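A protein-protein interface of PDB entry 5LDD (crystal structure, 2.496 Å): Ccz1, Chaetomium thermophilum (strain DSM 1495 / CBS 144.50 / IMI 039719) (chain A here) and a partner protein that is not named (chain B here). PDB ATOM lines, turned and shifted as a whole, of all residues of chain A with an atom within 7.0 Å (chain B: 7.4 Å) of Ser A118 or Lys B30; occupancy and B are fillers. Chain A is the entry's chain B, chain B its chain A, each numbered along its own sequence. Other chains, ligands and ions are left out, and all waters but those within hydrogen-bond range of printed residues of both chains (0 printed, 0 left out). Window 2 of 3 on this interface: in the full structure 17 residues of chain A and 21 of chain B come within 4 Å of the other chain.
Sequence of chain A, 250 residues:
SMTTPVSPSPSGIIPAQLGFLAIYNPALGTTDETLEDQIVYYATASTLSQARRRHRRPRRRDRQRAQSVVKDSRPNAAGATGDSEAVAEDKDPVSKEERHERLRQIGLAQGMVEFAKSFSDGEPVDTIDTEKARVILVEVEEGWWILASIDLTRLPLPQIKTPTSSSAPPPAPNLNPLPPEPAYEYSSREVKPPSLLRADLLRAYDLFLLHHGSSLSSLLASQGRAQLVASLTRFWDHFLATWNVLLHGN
The guanidinium group (NH2) of Arg B102 lies within hydrogen-bond range of the backbone carbonyl oxygen (O) of Phe A119, 3.2 Å away.
The side-chain amino group of Lys B30 lies close to the side-chain hydroxyl of Ser A118.
The side-chain hydroxyl (OG) of Ser A120 lies within hydrogen-bond range of the backbone carbonyl oxygen (O) of Glu A123, 2.6 Å away.
The backbone carbonyl oxygen (O) of Trp B29 sits at hydrogen-bond distance from a ring nitrogen (NE2) of His B35.
NH2 of Arg B102 is in hydrogen-bond range of O of Lys B32 (3.3 Å).
O of Leu B33 sits at hydrogen-bond distance from N of Arg B102, 2.7 Å away.
NH2 of Arg B102 sits at hydrogen-bond distance from O of Lys B30 (3.5 Å).
The side-chain hydroxyl of Ser A120 is in hydrogen-bond range of the backbone carbonyl oxygen of Ala A116.
Among the printed residues, pairs that only touch across the chains: Phe A115 with Phe B87 (3.6 Å), Ala A116 with Phe B87 (3.8 Å), Phe A119 with Trp B29 (3.8 Å), Phe A119 with Lys B30 (3.8 Å), Phe A119 with His B35 (3.9 Å), Phe A119 with Val B85 (3.4 Å) and Ser A120 with Val B85 (3.7 Å).
Ser A118 touches one residue of chain B.
Lys B30 touches two residues of chain A.
Of the printed residues of chain B, Ala A116 touches Phe B87 (3.8 Å).
Printed residues of chain B within 4 Å of Phe A119: Trp B29, Lys B30, His B35, Val B85 and Arg B102.
Of the printed residues of chain A, Arg B102 touches Phe A119.
Leu B28 touches none of the printed residues of chain A.
The nearest printed residue of chain B that does not touch Phe A115 is Thr B59 (4.03 Å).
Printed residues of chain A that touch a printed residue of chain B: Phe A115, Ala A116, Ser A118, Phe A119 and Ser A120.
Hydrophobic or aromatic side chains of chain A within 4 Å of the printed part of chain B: Phe A115, Ala A116 and Phe A119.
Along chain A the printed residues that touch a printed residue of chain B span positions 115 to 120.
Of the 18 printed residues of chain B, 6 touch a printed residue of chain A.
Hydrophobic or aromatic side chains of chain B within 4 Å of the printed part of chain A: Trp B29, His B35, Val B85 and Phe B87.
Among the printed residues, no Asp or Glu carboxylate lies within 4 Å of a Lys or Arg side-chain nitrogen of the other chain.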
ATOM      1  N   VAL A 113      -0.812 -11.584 -12.540  1.00  0.00           N
ATOM      2  CA  VAL A 113      -0.895 -11.349 -13.977  1.00  0.00           C
ATOM      3  C   VAL A 113      -0.969  -9.857 -14.274  1.00  0.00           C
ATOM      4  O   VAL A 113      -0.201  -9.326 -15.086  1.00  0.00           O
ATOM      5  CB  VAL A 113      -2.114 -12.087 -14.557  1.00  0.00           C
ATOM      6  CG1 VAL A 113      -2.426 -11.587 -15.968  1.00  0.00           C
ATOM      7  CG2 VAL A 113      -1.849 -13.558 -14.552  1.00  0.00           C
ATOM      8  N   GLU A 114      -1.900  -9.159 -13.617  1.00  0.00           N
ATOM      9  CA  GLU A 114      -2.039  -7.719 -13.828  1.00  0.00           C
ATOM     10  C   GLU A 114      -0.748  -6.987 -13.493  1.00  0.00           C
ATOM     11  O   GLU A 114      -0.308  -6.109 -14.241  1.00  0.00           O
ATOM     12  CB  GLU A 114      -3.187  -7.172 -12.983  1.00  0.00           C
ATOM     13  CG  GLU A 114      -3.501  -5.727 -13.227  1.00  0.00           C
ATOM     14  CD  GLU A 114      -3.918  -5.475 -14.661  1.00  0.00           C
ATOM     15  OE1 GLU A 114      -3.647  -4.368 -15.177  1.00  0.00           O
ATOM     16  OE2 GLU A 114      -4.529  -6.383 -15.267  1.00  0.00           O
ATOM     17  N   PHE A 115      -0.103  -7.371 -12.395  1.00  0.00           N
ATOM     18  CA  PHE A 115       1.117  -6.697 -11.980  1.00  0.00           C
ATOM     19  C   PHE A 115       2.242  -6.925 -12.983  1.00  0.00           C
ATOM     20  O   PHE A 115       2.888  -5.973 -13.439  1.00  0.00           O
ATOM     21  CB  PHE A 115       1.514  -7.183 -10.585  1.00  0.00           C
ATOM     22  CG  PHE A 115       2.891  -6.781 -10.174  1.00  0.00           C
ATOM     23  CD1 PHE A 115       3.149  -5.494  -9.757  1.00  0.00           C
ATOM     24  CD2 PHE A 115       3.935  -7.698 -10.213  1.00  0.00           C
ATOM     25  CE1 PHE A 115       4.427  -5.121  -9.376  1.00  0.00           C
ATOM     26  CE2 PHE A 115       5.224  -7.329  -9.835  1.00  0.00           C
ATOM     27  CZ  PHE A 115       5.467  -6.040  -9.416  1.00  0.00           C
ATOM     28  N   ALA A 116       2.470  -8.176 -13.367  1.00  0.00           N
ATOM     29  CA  ALA A 116       3.582  -8.472 -14.261  1.00  0.00           C
ATOM     30  C   ALA A 116       3.361  -7.936 -15.673  1.00  0.00           C
ATOM     31  O   ALA A 116       4.341  -7.648 -16.365  1.00  0.00           O
ATOM     32  CB  ALA A 116       3.841  -9.979 -14.302  1.00  0.00           C
ATOM     33  N   LYS A 117       2.112  -7.747 -16.107  1.00  0.00           N
ATOM     34  CA  LYS A 117       1.893  -7.238 -17.460  1.00  0.00           C
ATOM     35  C   LYS A 117       2.522  -5.862 -17.662  1.00  0.00           C
ATOM     36  O   LYS A 117       2.878  -5.504 -18.791  1.00  0.00           O
ATOM     37  CB  LYS A 117       0.402  -7.199 -17.787  1.00  0.00           C
ATOM     38  CG  LYS A 117      -0.145  -8.504 -18.354  1.00  0.00           C
ATOM     39  CD  LYS A 117      -1.641  -8.412 -18.619  1.00  0.00           C
ATOM     40  CE  LYS A 117      -2.162  -9.695 -19.245  1.00  0.00           C
ATOM     41  NZ  LYS A 117      -3.655  -9.706 -19.312  1.00  0.00           N
ATOM     42  N   SER A 118       2.692  -5.087 -16.587  1.00  0.00           N
ATOM     43  CA  SER A 118       3.328  -3.775 -16.709  1.00  0.00           C
ATOM     44  C   SER A 118       4.784  -3.894 -17.134  1.00  0.00           C
ATOM     45  O   SER A 118       5.315  -2.992 -17.793  1.00  0.00           O
ATOM     46  CB  SER A 118       3.267  -3.029 -15.378  1.00  0.00           C
ATOM     47  OG  SER A 118       1.958  -3.004 -14.854  1.00  0.00           O
ATOM     48  N   PHE A 119       5.442  -4.994 -16.776  1.00  0.00           N
ATOM     49  CA  PHE A 119       6.862  -5.154 -17.048  1.00  0.00           C
ATOM     50  C   PHE A 119       7.166  -6.069 -18.229  1.00  0.00           C
ATOM     51  O   PHE A 119       8.309  -6.072 -18.705  1.00  0.00           O
ATOM     52  CB  PHE A 119       7.578  -5.707 -15.810  1.00  0.00           C
ATOM     53  CG  PHE A 119       7.416  -4.862 -14.576  1.00  0.00           C
ATOM     54  CD1 PHE A 119       6.396  -5.111 -13.676  1.00  0.00           C
ATOM     55  CD2 PHE A 119       8.303  -3.832 -14.308  1.00  0.00           C
ATOM     56  CE1 PHE A 119       6.253  -4.346 -12.538  1.00  0.00           C
ATOM     57  CE2 PHE A 119       8.162  -3.056 -13.177  1.00  0.00           C
ATOM     58  CZ  PHE A 119       7.136  -3.310 -12.286  1.00  0.00           C
ATOM     59  N   SER A 120       6.193  -6.849 -18.706  1.00  0.00           N
ATOM     60  CA  SER A 120       6.456  -7.907 -19.672  1.00  0.00           C
ATOM     61  C   SER A 120       5.787  -7.669 -21.020  1.00  0.00           C
ATOM     62  O   SER A 120       5.557  -8.632 -21.764  1.00  0.00           O
ATOM     63  CB  SER A 120       5.999  -9.251 -19.111  1.00  0.00           C
ATOM     64  OG  SER A 120       4.582  -9.273 -19.029  1.00  0.00           O
ATOM     65  N   ASP A 121       5.450  -6.420 -21.345  1.00  0.00           N
ATOM     66  CA  ASP A 121       4.787  -6.113 -22.610  1.00  0.00           C
ATOM     67  C   ASP A 121       3.505  -6.932 -22.778  1.00  0.00           C
ATOM     68  O   ASP A 121       3.228  -7.482 -23.846  1.00  0.00           O
ATOM     69  CB  ASP A 121       5.735  -6.320 -23.794  1.00  0.00           C
ATOM     70  CG  ASP A 121       6.787  -5.222 -23.903  1.00  0.00           C
ATOM     71  OD1 ASP A 121       6.563  -4.253 -24.665  1.00  0.00           O
ATOM     72  OD2 ASP A 121       7.836  -5.324 -23.227  1.00  0.00           O
ATOM     73  N   GLY A 122       2.729  -7.044 -21.704  1.00  0.00           N
ATOM     74  CA  GLY A 122       1.443  -7.711 -21.742  1.00  0.00           C
ATOM     75  C   GLY A 122       1.455  -9.213 -21.554  1.00  0.00           C
ATOM     76  O   GLY A 122       0.385  -9.828 -21.625  1.00  0.00           O
ATOM     77  N   GLU A 123       2.614  -9.825 -21.308  1.00  0.00           N
ATOM     78  CA  GLU A 123       2.682 -11.281 -21.167  1.00  0.00           C
ATOM     79  C   GLU A 123       2.260 -11.713 -19.764  1.00  0.00           C
ATOM     80  O   GLU A 123       2.754 -11.168 -18.775  1.00  0.00           O
ATOM     81  CB  GLU A 123       4.092 -11.787 -21.451  1.00  0.00           C
ATOM     82  CG  GLU A 123       4.538 -11.591 -22.884  1.00  0.00           C
ATOM     83  CD  GLU A 123       3.588 -12.225 -23.883  1.00  0.00           C
ATOM     84  OE1 GLU A 123       3.169 -13.379 -23.657  1.00  0.00           O
ATOM     85  OE2 GLU A 123       3.259 -11.565 -24.893  1.00  0.00           O
ATOM     86  N   ILE B  16      15.406   8.848 -14.655  1.00  0.00           N
ATOM     87  CA  ILE B  16      14.082   9.246 -15.133  1.00  0.00           C
ATOM     88  C   ILE B  16      13.852  10.711 -14.779  1.00  0.00           C
ATOM     89  O   ILE B  16      13.918  11.079 -13.595  1.00  0.00           O
ATOM     90  CB  ILE B  16      12.973   8.356 -14.552  1.00  0.00           C
ATOM     91  CG1 ILE B  16      13.180   6.906 -14.985  1.00  0.00           C
ATOM     92  CG2 ILE B  16      11.614   8.843 -15.023  1.00  0.00           C
ATOM     93  CD1 ILE B  16      12.294   5.945 -14.267  1.00  0.00           C
ATOM     94  N   GLU B  24       4.714   9.697 -18.788  1.00  0.00           N
ATOM     95  CA  GLU B  24       5.963   9.277 -19.412  1.00  0.00           C
ATOM     96  C   GLU B  24       6.919   8.688 -18.387  1.00  0.00           C
ATOM     97  O   GLU B  24       7.575   7.674 -18.654  1.00  0.00           O
ATOM     98  CB  GLU B  24       6.609  10.456 -20.133  1.00  0.00           C
ATOM     99  CG  GLU B  24       5.714  11.098 -21.176  1.00  0.00           C
ATOM    100  CD  GLU B  24       6.299  12.382 -21.725  1.00  0.00           C
ATOM    101  OE1 GLU B  24       7.340  12.835 -21.199  1.00  0.00           O
ATOM    102  OE2 GLU B  24       5.712  12.942 -22.674  1.00  0.00           O
ATOM    103  N   ARG B  25       7.003   9.302 -17.204  1.00  0.00           N
ATOM    104  CA  ARG B  25       7.900   8.795 -16.175  1.00  0.00           C
ATOM    105  C   ARG B  25       7.542   7.364 -15.809  1.00  0.00           C
ATOM    106  O   ARG B  25       8.412   6.487 -15.750  1.00  0.00           O
ATOM    107  CB  ARG B  25       7.840   9.692 -14.942  1.00  0.00           C
ATOM    108  CG  ARG B  25       8.441  11.073 -15.122  1.00  0.00           C
ATOM    109  CD  ARG B  25       7.986  11.966 -13.989  1.00  0.00           C
ATOM    110  NE  ARG B  25       8.209  11.346 -12.691  1.00  0.00           N
ATOM    111  CZ  ARG B  25       7.729  11.826 -11.549  1.00  0.00           C
ATOM    112  NH1 ARG B  25       7.968  11.194 -10.411  1.00  0.00           N
ATOM    113  NH2 ARG B  25       6.989  12.929 -11.547  1.00  0.00           N
ATOM    114  N   LEU B  26       6.255   7.102 -15.582  1.00  0.00           N
ATOM    115  CA  LEU B  26       5.855   5.731 -15.297  1.00  0.00           C
ATOM    116  C   LEU B  26       6.096   4.833 -16.502  1.00  0.00           C
ATOM    117  O   LEU B  26       6.474   3.663 -16.338  1.00  0.00           O
ATOM    118  CB  LEU B  26       4.391   5.677 -14.850  1.00  0.00           C
ATOM    119  CG  LEU B  26       3.883   4.288 -14.409  1.00  0.00           C
ATOM    120  CD1 LEU B  26       4.728   3.710 -13.288  1.00  0.00           C
ATOM    121  CD2 LEU B  26       2.422   4.339 -13.977  1.00  0.00           C
ATOM    122  N   ALA B  27       5.935   5.374 -17.714  1.00  0.00           N
ATOM    123  CA  ALA B  27       6.234   4.592 -18.909  1.00  0.00           C
ATOM    124  C   ALA B  27       7.722   4.270 -18.992  1.00  0.00           C
ATOM    125  O   ALA B  27       8.105   3.110 -19.197  1.00  0.00           O
ATOM    126  CB  ALA B  27       5.781   5.353 -20.158  1.00  0.00           C
ATOM    127  N   LEU B  28       8.577   5.278 -18.788  1.00  0.00           N
ATOM    128  CA  LEU B  28      10.019   5.041 -18.797  1.00  0.00           C
ATOM    129  C   LEU B  28      10.419   4.041 -17.721  1.00  0.00           C
ATOM    130  O   LEU B  28      11.254   3.161 -17.960  1.00  0.00           O
ATOM    131  CB  LEU B  28      10.771   6.359 -18.602  1.00  0.00           C
ATOM    132  CG  LEU B  28      10.696   7.353 -19.756  1.00  0.00           C
ATOM    133  CD1 LEU B  28      11.367   8.660 -19.373  1.00  0.00           C
ATOM    134  CD2 LEU B  28      11.354   6.754 -20.989  1.00  0.00           C
ATOM    135  N   TRP B  29       9.826   4.152 -16.532  1.00  0.00           N
ATOM    136  CA  TRP B  29      10.181   3.253 -15.441  1.00  0.00           C
ATOM    137  C   TRP B  29       9.820   1.809 -15.780  1.00  0.00           C
ATOM    138  O   TRP B  29      10.652   0.906 -15.649  1.00  0.00           O
ATOM    139  CB  TRP B  29       9.487   3.690 -14.148  1.00  0.00           C
ATOM    140  CG  TRP B  29       9.967   2.956 -12.944  1.00  0.00           C
ATOM    141  CD1 TRP B  29      11.180   3.089 -12.339  1.00  0.00           C
ATOM    142  CD2 TRP B  29       9.268   1.946 -12.216  1.00  0.00           C
ATOM    143  NE1 TRP B  29      11.274   2.237 -11.264  1.00  0.00           N
ATOM    144  CE2 TRP B  29      10.112   1.522 -11.169  1.00  0.00           C
ATOM    145  CE3 TRP B  29       8.008   1.362 -12.342  1.00  0.00           C
ATOM    146  CZ2 TRP B  29       9.736   0.552 -10.255  1.00  0.00           C
ATOM    147  CZ3 TRP B  29       7.636   0.393 -11.435  1.00  0.00           C
ATOM    148  CH2 TRP B  29       8.496  -0.002 -10.402  1.00  0.00           C
ATOM    149  N   LYS B  30       8.583   1.576 -16.238  1.00  0.00           N
ATOM    150  CA  LYS B  30       8.151   0.224 -16.596  1.00  0.00           C
ATOM    151  C   LYS B  30       8.952  -0.371 -17.747  1.00  0.00           C
ATOM    152  O   LYS B  30       9.019  -1.599 -17.868  1.00  0.00           O
ATOM    153  CB  LYS B  30       6.665   0.209 -16.961  1.00  0.00           C
ATOM    154  CG  LYS B  30       5.730   0.548 -15.812  1.00  0.00           C
ATOM    155  CD  LYS B  30       5.808  -0.508 -14.712  1.00  0.00           C
ATOM    156  CE  LYS B  30       4.866  -0.191 -13.551  1.00  0.00           C
ATOM    157  NZ  LYS B  30       3.446  -0.035 -13.985  1.00  0.00           N
ATOM    158  N   GLY B  31       9.553   0.462 -18.595  1.00  0.00           N
ATOM    159  CA  GLY B  31      10.305  -0.052 -19.720  1.00  0.00           C
ATOM    160  C   GLY B  31      11.745  -0.436 -19.444  1.00  0.00           C
ATOM    161  O   GLY B  31      12.380  -1.046 -20.307  1.00  0.00           O
ATOM    162  N   LYS B  32      12.277  -0.091 -18.276  1.00  0.00           N
ATOM    163  CA  LYS B  32      13.655  -0.429 -17.941  1.00  0.00           C
ATOM    164  C   LYS B  32      13.871  -1.937 -18.059  1.00  0.00           C
ATOM    165  O   LYS B  32      12.942  -2.733 -17.910  1.00  0.00           O
ATOM    166  CB  LYS B  32      13.962   0.041 -16.523  1.00  0.00           C
ATOM    167  CG  LYS B  32      14.010   1.548 -16.395  1.00  0.00           C
ATOM    168  CD  LYS B  32      15.161   2.115 -17.193  1.00  0.00           C
ATOM    169  CE  LYS B  32      15.175   3.625 -17.164  1.00  0.00           C
ATOM    170  NZ  LYS B  32      16.320   4.150 -17.952  1.00  0.00           N
ATOM    171  N   LEU B  33      15.097  -2.332 -18.403  1.00  0.00           N
ATOM    172  CA  LEU B  33      15.359  -3.762 -18.536  1.00  0.00           C
ATOM    173  C   LEU B  33      15.528  -4.437 -17.186  1.00  0.00           C
ATOM    174  O   LEU B  33      15.189  -5.620 -17.038  1.00  0.00           O
ATOM    175  CB  LEU B  33      16.609  -4.004 -19.383  1.00  0.00           C
ATOM    176  CG  LEU B  33      16.550  -3.546 -20.838  1.00  0.00           C
ATOM    177  CD1 LEU B  33      17.908  -3.669 -21.483  1.00  0.00           C
ATOM    178  CD2 LEU B  33      15.561  -4.397 -21.585  1.00  0.00           C
ATOM    179  N   HIS B  35      15.229  -3.823 -12.834  1.00  0.00           N
ATOM    180  CA  HIS B  35      14.815  -3.084 -11.652  1.00  0.00           C
ATOM    181  C   HIS B  35      15.391  -3.744 -10.419  1.00  0.00           C
ATOM    182  O   HIS B  35      15.518  -4.973 -10.360  1.00  0.00           O
ATOM    183  CB  HIS B  35      13.293  -3.047 -11.504  1.00  0.00           C
ATOM    184  CG  HIS B  35      12.612  -2.155 -12.487  1.00  0.00           C
ATOM    185  ND1 HIS B  35      12.078  -2.621 -13.668  1.00  0.00           N
ATOM    186  CD2 HIS B  35      12.386  -0.819 -12.470  1.00  0.00           C
ATOM    187  CE1 HIS B  35      11.542  -1.614 -14.332  1.00  0.00           C
ATOM    188  NE2 HIS B  35      11.714  -0.510 -13.626  1.00  0.00           N
ATOM    189  N   LEU B  55       6.693   7.929  -7.319  1.00  0.00           N
ATOM    190  CA  LEU B  55       6.384   7.080  -8.459  1.00  0.00           C
ATOM    191  C   LEU B  55       6.361   5.591  -8.129  1.00  0.00           C
ATOM    192  O   LEU B  55       5.601   4.847  -8.750  1.00  0.00           O
ATOM    193  CB  LEU B  55       7.391   7.344  -9.578  1.00  0.00           C
ATOM    194  CG  LEU B  55       7.218   6.597 -10.897  1.00  0.00           C
ATOM    195  CD1 LEU B  55       7.465   7.538 -12.052  1.00  0.00           C
ATOM    196  CD2 LEU B  55       8.165   5.409 -10.958  1.00  0.00           C
ATOM    197  N   SER B  58       3.359   2.895  -4.944  1.00  0.00           N
ATOM    198  CA  SER B  58       2.217   2.013  -5.191  1.00  0.00           C
ATOM    199  C   SER B  58       2.683   0.633  -5.640  1.00  0.00           C
ATOM    200  O   SER B  58       2.127  -0.384  -5.211  1.00  0.00           O
ATOM    201  CB  SER B  58       1.263   2.632  -6.215  1.00  0.00           C
ATOM    202  OG  SER B  58       1.888   2.789  -7.476  1.00  0.00           O
ATOM    203  N   THR B  59       3.717   0.574  -6.484  1.00  0.00           N
ATOM    204  CA  THR B  59       4.294  -0.715  -6.861  1.00  0.00           C
ATOM    205  C   THR B  59       4.822  -1.460  -5.640  1.00  0.00           C
ATOM    206  O   THR B  59       4.687  -2.687  -5.541  1.00  0.00           O
ATOM    207  CB  THR B  59       5.413  -0.497  -7.885  1.00  0.00           C
ATOM    208  OG1 THR B  59       4.854  -0.033  -9.120  1.00  0.00           O
ATOM    209  CG2 THR B  59       6.246  -1.754  -8.100  1.00  0.00           C
ATOM    210  N   VAL B  85      10.442 -11.878 -18.830  1.00  0.00           N
ATOM    211  CA  VAL B  85      10.797 -11.185 -17.597  1.00  0.00           C
ATOM    212  C   VAL B  85      10.827 -12.153 -16.415  1.00  0.00           C
ATOM    213  O   VAL B  85       9.933 -12.987 -16.247  1.00  0.00           O
ATOM    214  CB  VAL B  85       9.812 -10.043 -17.319  1.00  0.00           C
ATOM    215  CG1 VAL B  85      10.232  -9.287 -16.079  1.00  0.00           C
ATOM    216  CG2 VAL B  85       9.730  -9.118 -18.528  1.00  0.00           C
ATOM    217  N   PHE B  87      11.197 -12.405 -12.160  1.00  0.00           N
ATOM    218  CA  PHE B  87      11.082 -11.762 -10.861  1.00  0.00           C
ATOM    219  C   PHE B  87      11.694 -12.686  -9.826  1.00  0.00           C
ATOM    220  O   PHE B  87      11.379 -13.881  -9.793  1.00  0.00           O
ATOM    221  CB  PHE B  87       9.616 -11.497 -10.487  1.00  0.00           C
ATOM    222  CG  PHE B  87       8.868 -10.658 -11.481  1.00  0.00           C
ATOM    223  CD1 PHE B  87       8.497 -11.174 -12.718  1.00  0.00           C
ATOM    224  CD2 PHE B  87       8.504  -9.360 -11.169  1.00  0.00           C
ATOM    225  CE1 PHE B  87       7.787 -10.398 -13.633  1.00  0.00           C
ATOM    226  CE2 PHE B  87       7.789  -8.581 -12.077  1.00  0.00           C
ATOM    227  CZ  PHE B  87       7.428  -9.097 -13.307  1.00  0.00           C
ATOM    228  N   ARG B 102      14.619  -8.268 -17.493  1.00  0.00           N
ATOM    229  CA  ARG B 102      14.347  -8.676 -18.862  1.00  0.00           C
ATOM    230  C   ARG B 102      15.603  -9.189 -19.560  1.00  0.00           C
ATOM    231  O   ARG B 102      15.552  -9.530 -20.746  1.00  0.00           O
ATOM    232  CB  ARG B 102      13.729  -7.513 -19.648  1.00  0.00           C
ATOM    233  CG  ARG B 102      12.921  -7.957 -20.852  1.00  0.00           C
ATOM    234  CD  ARG B 102      12.259  -6.790 -21.571  1.00  0.00           C
ATOM    235  NE  ARG B 102      11.388  -6.032 -20.680  1.00  0.00           N
ATOM    236  CZ  ARG B 102      11.432  -4.715 -20.537  1.00  0.00           C
ATOM    237  NH1 ARG B 102      12.296  -3.993 -21.239  1.00  0.00           N
ATOM    238  NH2 ARG B 102      10.601  -4.116 -19.698  1.00  0.00           N
